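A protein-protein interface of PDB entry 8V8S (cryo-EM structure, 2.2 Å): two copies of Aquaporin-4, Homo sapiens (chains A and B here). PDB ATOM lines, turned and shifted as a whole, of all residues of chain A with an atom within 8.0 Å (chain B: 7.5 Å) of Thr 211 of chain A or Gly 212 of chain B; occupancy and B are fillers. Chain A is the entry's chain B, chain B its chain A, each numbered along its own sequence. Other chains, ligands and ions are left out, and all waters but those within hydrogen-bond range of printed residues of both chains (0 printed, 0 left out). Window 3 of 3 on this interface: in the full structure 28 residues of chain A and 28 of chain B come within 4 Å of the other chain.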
ATOM      1  N   SER A 202      32.549  13.955  26.586  1.00  0.00           N
ATOM      2  CA  SER A 202      32.080  15.248  26.104  1.00  0.00           C
ATOM      3  C   SER A 202      32.519  15.541  24.676  1.00  0.00           C
ATOM      4  O   SER A 202      31.925  16.410  24.028  1.00  0.00           O
ATOM      5  CB  SER A 202      32.574  16.368  27.022  1.00  0.00           C
ATOM      6  OG  SER A 202      32.062  16.219  28.335  1.00  0.00           O
ATOM      7  N   ARG A 207      28.267  10.651  19.582  1.00  0.00           N
ATOM      8  CA  ARG A 207      27.149  10.988  20.450  1.00  0.00           C
ATOM      9  C   ARG A 207      26.246  12.030  19.801  1.00  0.00           C
ATOM     10  O   ARG A 207      26.683  12.853  18.992  1.00  0.00           O
ATOM     11  CB  ARG A 207      27.646  11.506  21.798  1.00  0.00           C
ATOM     12  CG  ARG A 207      28.266  10.446  22.689  1.00  0.00           C
ATOM     13  CD  ARG A 207      28.623  11.023  24.048  1.00  0.00           C
ATOM     14  NE  ARG A 207      27.435  11.359  24.824  1.00  0.00           N
ATOM     15  CZ  ARG A 207      27.451  11.750  26.091  1.00  0.00           C
ATOM     16  NH1 ARG A 207      28.584  11.864  26.765  1.00  0.00           N
ATOM     17  NH2 ARG A 207      26.302  12.031  26.698  1.00  0.00           N
ATOM     18  N   THR A 208      24.968  11.981  20.167  1.00  0.00           N
ATOM     19  CA  THR A 208      23.975  12.947  19.721  1.00  0.00           C
ATOM     20  C   THR A 208      23.326  13.711  20.866  1.00  0.00           C
ATOM     21  O   THR A 208      23.001  14.889  20.701  1.00  0.00           O
ATOM     22  CB  THR A 208      22.885  12.237  18.895  1.00  0.00           C
ATOM     23  OG1 THR A 208      23.461  11.716  17.691  1.00  0.00           O
ATOM     24  CG2 THR A 208      21.757  13.190  18.523  1.00  0.00           C
ATOM     25  N   ASP A 209      23.175  13.089  22.034  1.00  0.00           N
ATOM     26  CA  ASP A 209      22.482  13.680  23.171  1.00  0.00           C
ATOM     27  C   ASP A 209      23.349  14.637  23.981  1.00  0.00           C
ATOM     28  O   ASP A 209      22.989  14.954  25.120  1.00  0.00           O
ATOM     29  CB  ASP A 209      21.950  12.575  24.087  1.00  0.00           C
ATOM     30  CG  ASP A 209      23.049  11.652  24.583  1.00  0.00           C
ATOM     31  OD1 ASP A 209      23.655  10.945  23.750  1.00  0.00           O
ATOM     32  OD2 ASP A 209      23.308  11.636  25.804  1.00  0.00           O
ATOM     33  N   VAL A 210      24.471  15.099  23.439  1.00  0.00           N
ATOM     34  CA  VAL A 210      25.339  16.027  24.158  1.00  0.00           C
ATOM     35  C   VAL A 210      24.736  17.423  24.076  1.00  0.00           C
ATOM     36  O   VAL A 210      24.482  17.939  22.982  1.00  0.00           O
ATOM     37  CB  VAL A 210      26.764  16.005  23.591  1.00  0.00           C
ATOM     38  CG1 VAL A 210      27.612  17.079  24.252  1.00  0.00           C
ATOM     39  CG2 VAL A 210      27.389  14.635  23.786  1.00  0.00           C
ATOM     40  N   THR A 211      24.505  18.037  25.235  1.00  0.00           N
ATOM     41  CA  THR A 211      23.917  19.365  25.320  1.00  0.00           C
ATOM     42  C   THR A 211      24.772  20.244  26.223  1.00  0.00           C
ATOM     43  O   THR A 211      25.582  19.756  27.016  1.00  0.00           O
ATOM     44  CB  THR A 211      22.476  19.324  25.856  1.00  0.00           C
ATOM     45  OG1 THR A 211      22.481  18.888  27.222  1.00  0.00           O
ATOM     46  CG2 THR A 211      21.615  18.378  25.030  1.00  0.00           C
ATOM     47  N   GLY A 212      24.580  21.553  26.092  1.00  0.00           N
ATOM     48  CA  GLY A 212      25.277  22.506  26.926  1.00  0.00           C
ATOM     49  C   GLY A 212      26.703  22.762  26.476  1.00  0.00           C
ATOM     50  O   GLY A 212      27.146  22.351  25.398  1.00  0.00           O
ATOM     51  N   SER A 213      27.436  23.463  27.338  1.00  0.00           N
ATOM     52  CA  SER A 213      28.816  23.830  27.053  1.00  0.00           C
ATOM     53  C   SER A 213      29.739  22.667  27.403  1.00  0.00           C
ATOM     54  O   SER A 213      29.741  22.188  28.541  1.00  0.00           O
ATOM     55  CB  SER A 213      29.207  25.082  27.833  1.00  0.00           C
ATOM     56  OG  SER A 213      30.597  25.335  27.730  1.00  0.00           O
ATOM     57  N   ILE A 214      30.517  22.214  26.419  1.00  0.00           N
ATOM     58  CA  ILE A 214      31.482  21.148  26.669  1.00  0.00           C
ATOM     59  C   ILE A 214      32.565  21.622  27.631  1.00  0.00           C
ATOM     60  O   ILE A 214      32.969  20.889  28.541  1.00  0.00           O
ATOM     61  CB  ILE A 214      32.076  20.648  25.339  1.00  0.00           C
ATOM     62  CG1 ILE A 214      31.003  19.933  24.514  1.00  0.00           C
ATOM     63  CG2 ILE A 214      33.257  19.724  25.590  1.00  0.00           C
ATOM     64  CD1 ILE A 214      31.331  19.828  23.044  1.00  0.00           C
ATOM     65  N   ALA A 217      31.392  21.582  31.183  1.00  0.00           N
ATOM     66  CA  ALA A 217      31.335  20.232  31.734  1.00  0.00           C
ATOM     67  C   ALA A 217      32.715  19.757  32.173  1.00  0.00           C
ATOM     68  O   ALA A 217      32.849  19.085  33.203  1.00  0.00           O
ATOM     69  CB  ALA A 217      30.733  19.270  30.712  1.00  0.00           C
ATOM     70  N   GLN B 111      26.597  13.485  32.485  1.00  0.00           N
ATOM     71  CA  GLN B 111      27.353  13.800  31.278  1.00  0.00           C
ATOM     72  C   GLN B 111      28.212  12.616  30.845  1.00  0.00           C
ATOM     73  O   GLN B 111      28.321  12.323  29.650  1.00  0.00           O
ATOM     74  CB  GLN B 111      28.216  15.039  31.519  1.00  0.00           C
ATOM     75  CG  GLN B 111      29.470  15.115  30.667  1.00  0.00           C
ATOM     76  CD  GLN B 111      29.182  15.560  29.248  1.00  0.00           C
ATOM     77  OE1 GLN B 111      28.565  16.601  29.023  1.00  0.00           O
ATOM     78  NE2 GLN B 111      29.623  14.768  28.280  1.00  0.00           N
ATOM     79  N   ASP B 209      11.162  23.614  23.845  1.00  0.00           N
ATOM     80  CA  ASP B 209      11.801  24.777  24.449  1.00  0.00           C
ATOM     81  C   ASP B 209      12.907  24.418  25.435  1.00  0.00           C
ATOM     82  O   ASP B 209      13.304  25.276  26.229  1.00  0.00           O
ATOM     83  CB  ASP B 209      10.750  25.638  25.155  1.00  0.00           C
ATOM     84  CG  ASP B 209       9.984  24.868  26.215  1.00  0.00           C
ATOM     85  OD1 ASP B 209       9.253  23.921  25.853  1.00  0.00           O
ATOM     86  OD2 ASP B 209      10.114  25.207  27.409  1.00  0.00           O
ATOM     87  N   VAL B 210      13.411  23.188  25.412  1.00  0.00           N
ATOM     88  CA  VAL B 210      14.480  22.786  26.321  1.00  0.00           C
ATOM     89  C   VAL B 210      15.802  23.326  25.791  1.00  0.00           C
ATOM     90  O   VAL B 210      16.180  23.057  24.646  1.00  0.00           O
ATOM     91  CB  VAL B 210      14.527  21.260  26.480  1.00  0.00           C
ATOM     92  CG1 VAL B 210      15.734  20.854  27.310  1.00  0.00           C
ATOM     93  CG2 VAL B 210      13.244  20.755  27.118  1.00  0.00           C
ATOM     94  N   THR B 211      16.505  24.089  26.624  1.00  0.00           N
ATOM     95  CA  THR B 211      17.778  24.692  26.256  1.00  0.00           C
ATOM     96  C   THR B 211      18.816  24.386  27.327  1.00  0.00           C
ATOM     97  O   THR B 211      18.484  24.024  28.459  1.00  0.00           O
ATOM     98  CB  THR B 211      17.662  26.214  26.071  1.00  0.00           C
ATOM     99  OG1 THR B 211      17.368  26.832  27.331  1.00  0.00           O
ATOM    100  CG2 THR B 211      16.566  26.560  25.073  1.00  0.00           C
ATOM    101  N   GLY B 212      20.082  24.536  26.953  1.00  0.00           N
ATOM    102  CA  GLY B 212      21.173  24.339  27.881  1.00  0.00           C
ATOM    103  C   GLY B 212      21.508  22.875  28.108  1.00  0.00           C
ATOM    104  O   GLY B 212      21.032  21.970  27.416  1.00  0.00           O
ATOM    105  N   SER B 213      22.355  22.653  29.109  1.00  0.00           N
ATOM    106  CA  SER B 213      22.812  21.311  29.444  1.00  0.00           C
ATOM    107  C   SER B 213      21.778  20.622  30.326  1.00  0.00           C
ATOM    108  O   SER B 213      21.417  21.135  31.391  1.00  0.00           O
ATOM    109  CB  SER B 213      24.165  21.370  30.147  1.00  0.00           C
ATOM    110  OG  SER B 213      24.531  20.102  30.660  1.00  0.00           O
ATOM    111  N   ILE B 214      21.299  19.460  29.878  1.00  0.00           N
ATOM    112  CA  ILE B 214      20.353  18.690  30.679  1.00  0.00           C
ATOM    113  C   ILE B 214      21.017  18.197  31.960  1.00  0.00           C
ATOM    114  O   ILE B 214      20.417  18.239  33.041  1.00  0.00           O
ATOM    115  CB  ILE B 214      19.777  17.528  29.848  1.00  0.00           C
ATOM    116  CG1 ILE B 214      18.891  18.070  28.725  1.00  0.00           C
ATOM    117  CG2 ILE B 214      18.991  16.572  30.731  1.00  0.00           C
ATOM    118  CD1 ILE B 214      18.668  17.091  27.596  1.00  0.00           C
ATOM    119  N   ALA B 215      22.265  17.732  31.862  1.00  0.00           N
ATOM    120  CA  ALA B 215      22.968  17.236  33.040  1.00  0.00           C
ATOM    121  C   ALA B 215      23.167  18.340  34.072  1.00  0.00           C
ATOM    122  O   ALA B 215      23.039  18.101  35.278  1.00  0.00           O
ATOM    123  CB  ALA B 215      24.313  16.633  32.636  1.00  0.00           C
ATOM    124  N   LEU B 216      23.484  19.554  33.617  1.00  0.00           N
ATOM    125  CA  LEU B 216      23.667  20.664  34.547  1.00  0.00           C
ATOM    126  C   LEU B 216      22.363  21.047  35.234  1.00  0.00           C
ATOM    127  O   LEU B 216      22.381  21.495  36.386  1.00  0.00           O
ATOM    128  CB  LEU B 216      24.262  21.867  33.816  1.00  0.00           C
ATOM    129  CG  LEU B 216      24.993  22.888  34.688  1.00  0.00           C
ATOM    130  CD1 LEU B 216      25.856  22.187  35.725  1.00  0.00           C
ATOM    131  CD2 LEU B 216      25.835  23.815  33.829  1.00  0.00           C
ATOM    132  N   ALA B 217      21.229  20.888  34.549  1.00  0.00           N
ATOM    133  CA  ALA B 217      19.942  21.151  35.184  1.00  0.00           C
ATOM    134  C   ALA B 217      19.638  20.121  36.264  1.00  0.00           C
ATOM    135  O   ALA B 217      19.088  20.462  37.318  1.00  0.00           O
ATOM    136  CB  ALA B 217      18.833  21.177  34.134  1.00  0.00           C
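Thr 211 of chain A touches Ser 213 of chain B.
Gly 212 of chain B touches Gly 212 of chain A.
Ser 213 of chain B touches Gly 212 of chain A (CB to CA, 3.6 Å).
Gln 111 of chain B touches Ala 217 of chain A.
NE2 of Gln 111 of chain B is in hydrogen-bond range of OG of Ser 202 of chain A (2.8 Å).
The backbone carbonyl oxygen (O) of Gln 111 of chain B is in hydrogen-bond range of the guanidinium group (NH1) of Arg 207 of chain A, at 2.9 Å.
The backbone carbonyl oxygen (O) of Gly 212 of chain B lies close to the side-chain hydroxyl (OG1) of Thr 211 of chain A.
The side-chain hydroxyl (OG1) of Thr 211 of chain A lies within hydrogen-bond range of the backbone NH (N) of Ile 214 of chain B, 3.0 Å away.
Thr 211 of chain A touches Ser 213 of chain B, but with the chains exchanged Ser 213 of chain A does not touch Thr 211 of chain B (8.7 Å).
Thr 211 of chain A touches Ile 214 of chain B, but with the chains exchanged Ile 214 of chain A does not touch Thr 211 of chain B (11.9 Å).
Gly 212 of chain A touches its own counterpart, Gly 212 of chain B.
Gly 212 of chain A touches Ser 213 of chain B, but with the chains exchanged Ser 213 of chain A does not touch Gly 212 of chain B (6.0 Å).
The side-chain hydroxyl (OG) of Ser 213 of chain B sits close to the backbone NH (N) of Ala 215 of chain B (3.5 Å).
OG of Ser 213 of chain B sits at hydrogen-bond distance from N of Leu 216 of chain B (3.2 Å).
The guanidinium group of Arg 207 of chain A lies within salt-bridge range of the side-chain carboxylate of Asp 209 of chain A, at 3.1 Å.
Of the 10 printed residues of chain B, 4 touch a printed residue of chain A.
Of the 10 printed residues of chain A, 5 touch a printed residue of chain B.
Hydrophobic or aromatic side chains of chain A within 4 Å of the printed part of chain B: Ala 217.
Among the printed residues, 8 pairs touch across the chains.
Among the printed residues, no Asp or Glu carboxylate lies within 4 Å of a Lys or Arg side-chain nitrogen of the other chain.
Printed residues of chain B within 4 Å of Ser 202 of chain A: Gln 111.
Of the printed residues of chain B, Arg 207 of chain A touches Gln 111 (2.9 Å).
Asp 209 of chain A touches none of the printed residues of chain B.
Of chain B, only Gly 212 (3.4 Å), Ser 213 (3.3 Å) and Ile 214 (3.0 Å) come within 4 Å of Thr 211 of chain A.
Of the printed residues of chain B, Ala 217 of chain A touches Gln 111.
Of the printed residues of chain A, Gln 111 of chain B touches Ser 202, Arg 207 and Ala 217.
Asp 209 of chain B touches none of the printed residues of chain A.
Of chain A, only Thr 211 and Gly 212 come within 4 Å of Gly 212 of chain B.
Ser 213 of chain B touches just these residues of chain A: Thr 211 (3.3 Å) and Gly 212 (3.6 Å).
Printed residues of chain A within 4 Å of Ile 214 of chain B: Thr 211.
The nearest printed residue of chain B that does not touch Thr 211 of chain A is Gln 111 of chain B (4.8 Å).
The nearest printed residue of chain B that does not touch Ser 202 of chain A is Ser 213 of chain B (8.8 Å).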
